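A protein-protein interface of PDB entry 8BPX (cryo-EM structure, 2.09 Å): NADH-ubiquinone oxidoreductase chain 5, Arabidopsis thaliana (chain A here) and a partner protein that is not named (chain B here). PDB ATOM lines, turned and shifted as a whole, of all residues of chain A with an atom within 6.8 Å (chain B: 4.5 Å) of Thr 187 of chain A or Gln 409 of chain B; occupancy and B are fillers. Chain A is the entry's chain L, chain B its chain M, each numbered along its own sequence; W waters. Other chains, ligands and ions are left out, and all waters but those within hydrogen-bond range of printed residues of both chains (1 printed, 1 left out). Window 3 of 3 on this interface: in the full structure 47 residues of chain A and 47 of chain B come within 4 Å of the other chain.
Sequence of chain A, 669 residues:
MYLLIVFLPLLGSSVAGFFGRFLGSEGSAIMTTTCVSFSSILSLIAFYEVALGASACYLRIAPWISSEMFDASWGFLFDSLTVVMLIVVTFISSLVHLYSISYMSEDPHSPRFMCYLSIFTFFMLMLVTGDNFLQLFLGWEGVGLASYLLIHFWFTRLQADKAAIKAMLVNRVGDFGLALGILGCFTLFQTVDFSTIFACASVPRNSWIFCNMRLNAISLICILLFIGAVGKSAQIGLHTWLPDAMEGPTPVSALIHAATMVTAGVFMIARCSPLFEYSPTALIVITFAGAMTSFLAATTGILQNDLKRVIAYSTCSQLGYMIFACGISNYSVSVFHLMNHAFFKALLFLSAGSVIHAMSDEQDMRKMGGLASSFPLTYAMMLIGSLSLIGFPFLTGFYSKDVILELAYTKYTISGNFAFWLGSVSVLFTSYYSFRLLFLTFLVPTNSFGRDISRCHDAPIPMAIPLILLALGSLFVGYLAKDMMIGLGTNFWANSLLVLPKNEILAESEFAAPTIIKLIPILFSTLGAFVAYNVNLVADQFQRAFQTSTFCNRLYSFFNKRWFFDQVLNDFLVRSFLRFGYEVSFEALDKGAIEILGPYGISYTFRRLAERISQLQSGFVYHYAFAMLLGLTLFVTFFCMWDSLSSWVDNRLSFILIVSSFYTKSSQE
Of the 13 printed residues of chain A, 6 touch a printed residue of chain B.
Of the 8 printed residues of chain B, 4 touch a printed residue of chain A.
Hydrophobic or aromatic side chains of chain B within 4 Å of the printed part of chain A: Val 405 and Phe 408.
Among the printed residues, no Asp or Glu carboxylate lies within 4 Å of a Lys or Arg side-chain nitrogen of the other chain.
Water W1 lies within hydrogen-bond range of OE1 of Glu 68 of chain A (3.0 Å) and OE1 of Gln 329 of chain B (3.0 Å).
The side-chain amide nitrogen (NE2) of Gln 409 of chain B is in hydrogen-bond range of the side-chain amide oxygen (OE1) of Gln 329 of chain B (3.3 Å).
The side-chain amide nitrogen of Gln 409 of chain B sits at hydrogen-bond distance from the backbone carbonyl oxygen of Val 405 of chain B.
O of Phe 186 of chain A lies close to NE2 of Gln 190 of chain A (3.4 Å).
O of Leu 183 of chain A is in hydrogen-bond range of OG1 of Thr 187 of chain A (2.9 Å).
O of Thr 187 of chain A lies within hydrogen-bond range of NE2 of Gln 190 of chain A, at 3.5 Å.
Printed residues of chain B within 4 Å of Thr 187 of chain A: Phe 408 (3.3 Å) and Gln 409 (3.8 Å).
Printed residues of chain B within 4 Å of Gln 190 of chain A: Gln 409.
Thr 191 of chain A touches none of the printed residues of chain B.
Trp 208 of chain A touches none of the printed residues of chain B.
Printed residues of chain A within 4 Å of Gln 329 of chain B: Glu 68.
Of the printed residues of chain A, Phe 408 of chain B touches Leu 183 (3.9 Å), Gly 184 (3.7 Å) and Thr 187 (3.3 Å).
The nearest printed residue of chain B that does not touch Thr 187 of chain A is Val 405 of chain B (5.3 Å).
The nearest printed residue of chain B that does not touch Glu 68 of chain A is Gln 409 of chain B (5.7 Å).
Among the printed residues, merely in contact across the chains: Thr 187 of chain A with Phe 408 of chain B, Leu 183 of chain A with Val 405 of chain B, Phe 186 of chain A with Val 405 of chain B, Gln 190 of chain A with Gln 409 of chain B, Glu 68 of chain A with Gln 329 of chain B, Gly 184 of chain A with Phe 408 of chain B, Thr 187 of chain A with Gln 409 of chain B, Phe 186 of chain A with Gln 409 of chain B and Leu 183 of chain A with Phe 408 of chain B.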
ATOM      1  N   GLU A  68      -4.199 -30.982 -12.581  1.00  0.00           N
ATOM      2  CA  GLU A  68      -3.954 -31.963 -11.487  1.00  0.00           C
ATOM      3  C   GLU A  68      -5.269 -32.707 -11.207  1.00  0.00           C
ATOM      4  O   GLU A  68      -5.852 -33.243 -12.163  1.00  0.00           O
ATOM      5  CB  GLU A  68      -3.394 -31.245 -10.254  1.00  0.00           C
ATOM      6  CG  GLU A  68      -2.661 -32.148  -9.283  1.00  0.00           C
ATOM      7  CD  GLU A  68      -2.727 -31.699  -7.834  1.00  0.00           C
ATOM      8  OE1 GLU A  68      -1.777 -31.034  -7.378  1.00  0.00           O
ATOM      9  OE2 GLU A  68      -3.727 -32.021  -7.163  1.00  0.00           O
ATOM     10  N   ILE A 182     -18.828 -24.856  -4.482  1.00  0.00           N
ATOM     11  CA  ILE A 182     -18.124 -25.722  -5.424  1.00  0.00           C
ATOM     12  C   ILE A 182     -16.659 -25.865  -5.028  1.00  0.00           C
ATOM     13  O   ILE A 182     -16.076 -26.955  -5.117  1.00  0.00           O
ATOM     14  CB  ILE A 182     -18.286 -25.189  -6.859  1.00  0.00           C
ATOM     15  CG1 ILE A 182     -19.762 -25.221  -7.271  1.00  0.00           C
ATOM     16  CG2 ILE A 182     -17.415 -25.970  -7.836  1.00  0.00           C
ATOM     17  CD1 ILE A 182     -20.005 -24.988  -8.730  1.00  0.00           C
ATOM     18  N   LEU A 183     -16.043 -24.766  -4.587  1.00  0.00           N
ATOM     19  CA  LEU A 183     -14.664 -24.833  -4.118  1.00  0.00           C
ATOM     20  C   LEU A 183     -14.547 -25.779  -2.930  1.00  0.00           C
ATOM     21  O   LEU A 183     -13.625 -26.598  -2.864  1.00  0.00           O
ATOM     22  CB  LEU A 183     -14.167 -23.438  -3.738  1.00  0.00           C
ATOM     23  CG  LEU A 183     -14.097 -22.402  -4.866  1.00  0.00           C
ATOM     24  CD1 LEU A 183     -13.790 -21.011  -4.321  1.00  0.00           C
ATOM     25  CD2 LEU A 183     -13.139 -22.793  -5.946  1.00  0.00           C
ATOM     26  N   GLY A 184     -15.486 -25.684  -1.985  1.00  0.00           N
ATOM     27  CA  GLY A 184     -15.471 -26.592  -0.850  1.00  0.00           C
ATOM     28  C   GLY A 184     -15.649 -28.045  -1.256  1.00  0.00           C
ATOM     29  O   GLY A 184     -14.983 -28.934  -0.720  1.00  0.00           O
ATOM     30  N   CYS A 185     -16.549 -28.300  -2.207  1.00  0.00           N
ATOM     31  CA  CYS A 185     -16.738 -29.654  -2.720  1.00  0.00           C
ATOM     32  C   CYS A 185     -15.443 -30.209  -3.294  1.00  0.00           C
ATOM     33  O   CYS A 185     -15.039 -31.336  -2.974  1.00  0.00           O
ATOM     34  CB  CYS A 185     -17.835 -29.670  -3.787  1.00  0.00           C
ATOM     35  SG  CYS A 185     -19.457 -30.180  -3.214  1.00  0.00           S
ATOM     36  N   PHE A 186     -14.773 -29.428  -4.146  1.00  0.00           N
ATOM     37  CA  PHE A 186     -13.517 -29.903  -4.714  1.00  0.00           C
ATOM     38  C   PHE A 186     -12.476 -30.143  -3.632  1.00  0.00           C
ATOM     39  O   PHE A 186     -11.723 -31.116  -3.693  1.00  0.00           O
ATOM     40  CB  PHE A 186     -12.943 -28.931  -5.737  1.00  0.00           C
ATOM     41  CG  PHE A 186     -11.612 -29.370  -6.253  1.00  0.00           C
ATOM     42  CD1 PHE A 186     -11.505 -30.515  -7.029  1.00  0.00           C
ATOM     43  CD2 PHE A 186     -10.451 -28.715  -5.869  1.00  0.00           C
ATOM     44  CE1 PHE A 186     -10.282 -30.953  -7.475  1.00  0.00           C
ATOM     45  CE2 PHE A 186      -9.220 -29.153  -6.312  1.00  0.00           C
ATOM     46  CZ  PHE A 186      -9.132 -30.272  -7.114  1.00  0.00           C
ATOM     47  N   THR A 187     -12.393 -29.250  -2.649  1.00  0.00           N
ATOM     48  CA  THR A 187     -11.381 -29.424  -1.615  1.00  0.00           C
ATOM     49  C   THR A 187     -11.628 -30.696  -0.812  1.00  0.00           C
ATOM     50  O   THR A 187     -10.685 -31.424  -0.485  1.00  0.00           O
ATOM     51  CB  THR A 187     -11.345 -28.203  -0.699  1.00  0.00           C
ATOM     52  OG1 THR A 187     -11.137 -27.027  -1.488  1.00  0.00           O
ATOM     53  CG2 THR A 187     -10.224 -28.333   0.303  1.00  0.00           C
ATOM     54  N   LEU A 188     -12.889 -30.988  -0.499  1.00  0.00           N
ATOM     55  CA  LEU A 188     -13.190 -32.166   0.308  1.00  0.00           C
ATOM     56  C   LEU A 188     -13.002 -33.458  -0.483  1.00  0.00           C
ATOM     57  O   LEU A 188     -12.392 -34.412   0.013  1.00  0.00           O
ATOM     58  CB  LEU A 188     -14.610 -32.075   0.859  1.00  0.00           C
ATOM     59  CG  LEU A 188     -14.987 -33.158   1.872  1.00  0.00           C
ATOM     60  CD1 LEU A 188     -14.006 -33.192   3.030  1.00  0.00           C
ATOM     61  CD2 LEU A 188     -16.391 -32.924   2.370  1.00  0.00           C
ATOM     62  N   PHE A 189     -13.509 -33.514  -1.713  1.00  0.00           N
ATOM     63  CA  PHE A 189     -13.524 -34.764  -2.464  1.00  0.00           C
ATOM     64  C   PHE A 189     -12.451 -34.847  -3.543  1.00  0.00           C
ATOM     65  O   PHE A 189     -12.248 -35.930  -4.103  1.00  0.00           O
ATOM     66  CB  PHE A 189     -14.904 -34.983  -3.100  1.00  0.00           C
ATOM     67  CG  PHE A 189     -16.032 -35.017  -2.106  1.00  0.00           C
ATOM     68  CD1 PHE A 189     -16.283 -36.157  -1.359  1.00  0.00           C
ATOM     69  CD2 PHE A 189     -16.840 -33.909  -1.914  1.00  0.00           C
ATOM     70  CE1 PHE A 189     -17.318 -36.190  -0.443  1.00  0.00           C
ATOM     71  CE2 PHE A 189     -17.878 -33.936  -1.002  1.00  0.00           C
ATOM     72  CZ  PHE A 189     -18.114 -35.077  -0.264  1.00  0.00           C
ATOM     73  N   GLN A 190     -11.722 -33.782  -3.845  1.00  0.00           N
ATOM     74  CA  GLN A 190     -10.714 -33.775  -4.956  1.00  0.00           C
ATOM     75  C   GLN A 190     -11.404 -34.069  -6.291  1.00  0.00           C
ATOM     76  O   GLN A 190     -10.798 -34.629  -7.134  1.00  0.00           O
ATOM     77  CB  GLN A 190      -9.468 -34.594  -4.612  1.00  0.00           C
ATOM     78  CG  GLN A 190      -8.665 -34.006  -3.457  1.00  0.00           C
ATOM     79  CD  GLN A 190      -7.993 -32.687  -3.760  1.00  0.00           C
ATOM     80  OE1 GLN A 190      -7.071 -32.612  -4.556  1.00  0.00           O
ATOM     81  NE2 GLN A 190      -8.438 -31.633  -3.102  1.00  0.00           N
ATOM     82  N   THR A 191     -12.624 -33.628  -6.455  1.00  0.00           N
ATOM     83  CA  THR A 191     -13.300 -33.765  -7.735  1.00  0.00           C
ATOM     84  C   THR A 191     -14.489 -32.820  -7.757  1.00  0.00           C
ATOM     85  O   THR A 191     -14.957 -32.358  -6.714  1.00  0.00           O
ATOM     86  CB  THR A 191     -13.751 -35.212  -7.989  1.00  0.00           C
ATOM     87  OG1 THR A 191     -14.321 -35.319  -9.296  1.00  0.00           O
ATOM     88  CG2 THR A 191     -14.769 -35.646  -6.956  1.00  0.00           C
ATOM     89  N   TRP A 208     -13.747 -28.154   9.377  1.00  0.00           N
ATOM     90  CA  TRP A 208     -13.023 -27.219   8.539  1.00  0.00           C
ATOM     91  C   TRP A 208     -12.927 -25.873   9.236  1.00  0.00           C
ATOM     92  O   TRP A 208     -13.745 -25.528  10.090  1.00  0.00           O
ATOM     93  CB  TRP A 208     -13.699 -27.056   7.180  1.00  0.00           C
ATOM     94  CG  TRP A 208     -13.153 -27.960   6.147  1.00  0.00           C
ATOM     95  CD1 TRP A 208     -12.207 -28.921   6.321  1.00  0.00           C
ATOM     96  CD2 TRP A 208     -13.543 -28.021   4.777  1.00  0.00           C
ATOM     97  NE1 TRP A 208     -11.969 -29.570   5.136  1.00  0.00           N
ATOM     98  CE2 TRP A 208     -12.781 -29.037   4.172  1.00  0.00           C
ATOM     99  CE3 TRP A 208     -14.460 -27.314   4.000  1.00  0.00           C
ATOM    100  CZ2 TRP A 208     -12.908 -29.362   2.825  1.00  0.00           C
ATOM    101  CZ3 TRP A 208     -14.583 -27.637   2.664  1.00  0.00           C
ATOM    102  CH2 TRP A 208     -13.812 -28.650   2.091  1.00  0.00           C
ATOM    103  N   ILE A 221     -20.447 -26.864   3.006  1.00  0.00           N
ATOM    104  CA  ILE A 221     -20.616 -26.978   1.563  1.00  0.00           C
ATOM    105  C   ILE A 221     -22.091 -26.865   1.191  1.00  0.00           C
ATOM    106  O   ILE A 221     -22.465 -26.144   0.257  1.00  0.00           O
ATOM    107  CB  ILE A 221     -20.007 -28.301   1.063  1.00  0.00           C
ATOM    108  CG1 ILE A 221     -18.490 -28.179   0.925  1.00  0.00           C
ATOM    109  CG2 ILE A 221     -20.629 -28.713  -0.256  1.00  0.00           C
ATOM    110  CD1 ILE A 221     -17.759 -29.491   1.079  1.00  0.00           C
ATOM    111  N   GLN B 329      -3.273 -25.360  -9.118  1.00  0.00           N
ATOM    112  CA  GLN B 329      -4.407 -24.489  -9.429  1.00  0.00           C
ATOM    113  C   GLN B 329      -3.976 -23.016  -9.293  1.00  0.00           C
ATOM    114  O   GLN B 329      -4.227 -22.297 -10.224  1.00  0.00           O
ATOM    115  CB  GLN B 329      -5.664 -24.878  -8.661  1.00  0.00           C
ATOM    116  CG  GLN B 329      -6.106 -26.308  -8.951  1.00  0.00           C
ATOM    117  CD  GLN B 329      -5.448 -27.378  -8.107  1.00  0.00           C
ATOM    118  OE1 GLN B 329      -4.978 -27.137  -7.007  1.00  0.00           O
ATOM    119  NE2 GLN B 329      -5.436 -28.593  -8.615  1.00  0.00           N
ATOM    120  N   VAL B 405      -9.704 -21.784  -6.582  1.00  0.00           N
ATOM    121  CA  VAL B 405      -9.447 -23.154  -6.131  1.00  0.00           C
ATOM    122  C   VAL B 405      -8.132 -23.221  -5.369  1.00  0.00           C
ATOM    123  O   VAL B 405      -8.055 -23.793  -4.276  1.00  0.00           O
ATOM    124  CB  VAL B 405      -9.432 -24.134  -7.321  1.00  0.00           C
ATOM    125  CG1 VAL B 405      -8.925 -25.498  -6.873  1.00  0.00           C
ATOM    126  CG2 VAL B 405     -10.797 -24.269  -7.959  1.00  0.00           C
ATOM    127  N   GLY B 406      -7.079 -22.630  -5.937  1.00  0.00           N
ATOM    128  CA  GLY B 406      -5.782 -22.664  -5.286  1.00  0.00           C
ATOM    129  C   GLY B 406      -5.786 -21.968  -3.941  1.00  0.00           C
ATOM    130  O   GLY B 406      -5.184 -22.448  -2.980  1.00  0.00           O
ATOM    131  N   ALA B 407      -6.482 -20.833  -3.851  1.00  0.00           N
ATOM    132  CA  ALA B 407      -6.523 -20.078  -2.605  1.00  0.00           C
ATOM    133  C   ALA B 407      -7.345 -20.796  -1.543  1.00  0.00           C
ATOM    134  O   ALA B 407      -6.971 -20.801  -0.367  1.00  0.00           O
ATOM    135  CB  ALA B 407      -7.082 -18.679  -2.858  1.00  0.00           C
ATOM    136  N   PHE B 408      -8.462 -21.412  -1.938  1.00  0.00           N
ATOM    137  CA  PHE B 408      -9.341 -22.054  -0.966  1.00  0.00           C
ATOM    138  C   PHE B 408      -8.630 -23.189  -0.241  1.00  0.00           C
ATOM    139  O   PHE B 408      -8.822 -23.380   0.964  1.00  0.00           O
ATOM    140  CB  PHE B 408     -10.605 -22.569  -1.654  1.00  0.00           C
ATOM    141  CG  PHE B 408     -11.730 -22.855  -0.707  1.00  0.00           C
ATOM    142  CD1 PHE B 408     -11.873 -24.111  -0.139  1.00  0.00           C
ATOM    143  CD2 PHE B 408     -12.642 -21.869  -0.380  1.00  0.00           C
ATOM    144  CE1 PHE B 408     -12.904 -24.375   0.737  1.00  0.00           C
ATOM    145  CE2 PHE B 408     -13.675 -22.129   0.493  1.00  0.00           C
ATOM    146  CZ  PHE B 408     -13.807 -23.389   1.051  1.00  0.00           C
ATOM    147  N   GLN B 409      -7.801 -23.948  -0.957  1.00  0.00           N
ATOM    148  CA  GLN B 409      -7.084 -25.051  -0.332  1.00  0.00           C
ATOM    149  C   GLN B 409      -6.055 -24.585   0.691  1.00  0.00           C
ATOM    150  O   GLN B 409      -5.697 -25.362   1.578  1.00  0.00           O
ATOM    151  CB  GLN B 409      -6.421 -25.916  -1.402  1.00  0.00           C
ATOM    152  CG  GLN B 409      -7.394 -26.855  -2.092  1.00  0.00           C
ATOM    153  CD  GLN B 409      -6.901 -27.329  -3.439  1.00  0.00           C
ATOM    154  OE1 GLN B 409      -6.520 -28.487  -3.599  1.00  0.00           O
ATOM    155  NE2 GLN B 409      -6.912 -26.440  -4.419  1.00  0.00           N
ATOM    156  N   ARG B 410      -5.589 -23.340   0.604  1.00  0.00           N
ATOM    157  CA  ARG B 410      -4.637 -22.814   1.575  1.00  0.00           C
ATOM    158  C   ARG B 410      -5.329 -22.038   2.692  1.00  0.00           C
ATOM    159  O   ARG B 410      -5.055 -22.266   3.871  1.00  0.00           O
ATOM    160  CB  ARG B 410      -3.607 -21.911   0.884  1.00  0.00           C
ATOM    161  CG  ARG B 410      -2.755 -22.604  -0.150  1.00  0.00           C
ATOM    162  CD  ARG B 410      -1.632 -23.411   0.478  1.00  0.00           C
ATOM    163  NE  ARG B 410      -1.099 -22.802   1.690  1.00  0.00           N
ATOM    164  CZ  ARG B 410      -0.100 -21.930   1.718  1.00  0.00           C
ATOM    165  NH1 ARG B 410       0.487 -21.514   0.609  1.00  0.00           N
ATOM    166  NH2 ARG B 410       0.318 -21.463   2.889  1.00  0.00           N
ATOM    167  N   ASN B 411      -6.203 -21.105   2.328  1.00  0.00           N
ATOM    168  CA  ASN B 411      -6.858 -20.217   3.286  1.00  0.00           C
ATOM    169  C   ASN B 411      -8.255 -19.916   2.767  1.00  0.00           C
ATOM    170  O   ASN B 411      -8.401 -19.263   1.730  1.00  0.00           O
ATOM    171  CB  ASN B 411      -6.056 -18.931   3.476  1.00  0.00           C
ATOM    172  CG  ASN B 411      -6.155 -18.387   4.882  1.00  0.00           C
ATOM    173  OD1 ASN B 411      -7.153 -17.767   5.242  1.00  0.00           O
ATOM    174  ND2 ASN B 411      -5.122 -18.610   5.685  1.00  0.00           N
HETATM  175  O   HOH W   1      -2.341 -28.346  -6.207  1.00  0.00           O
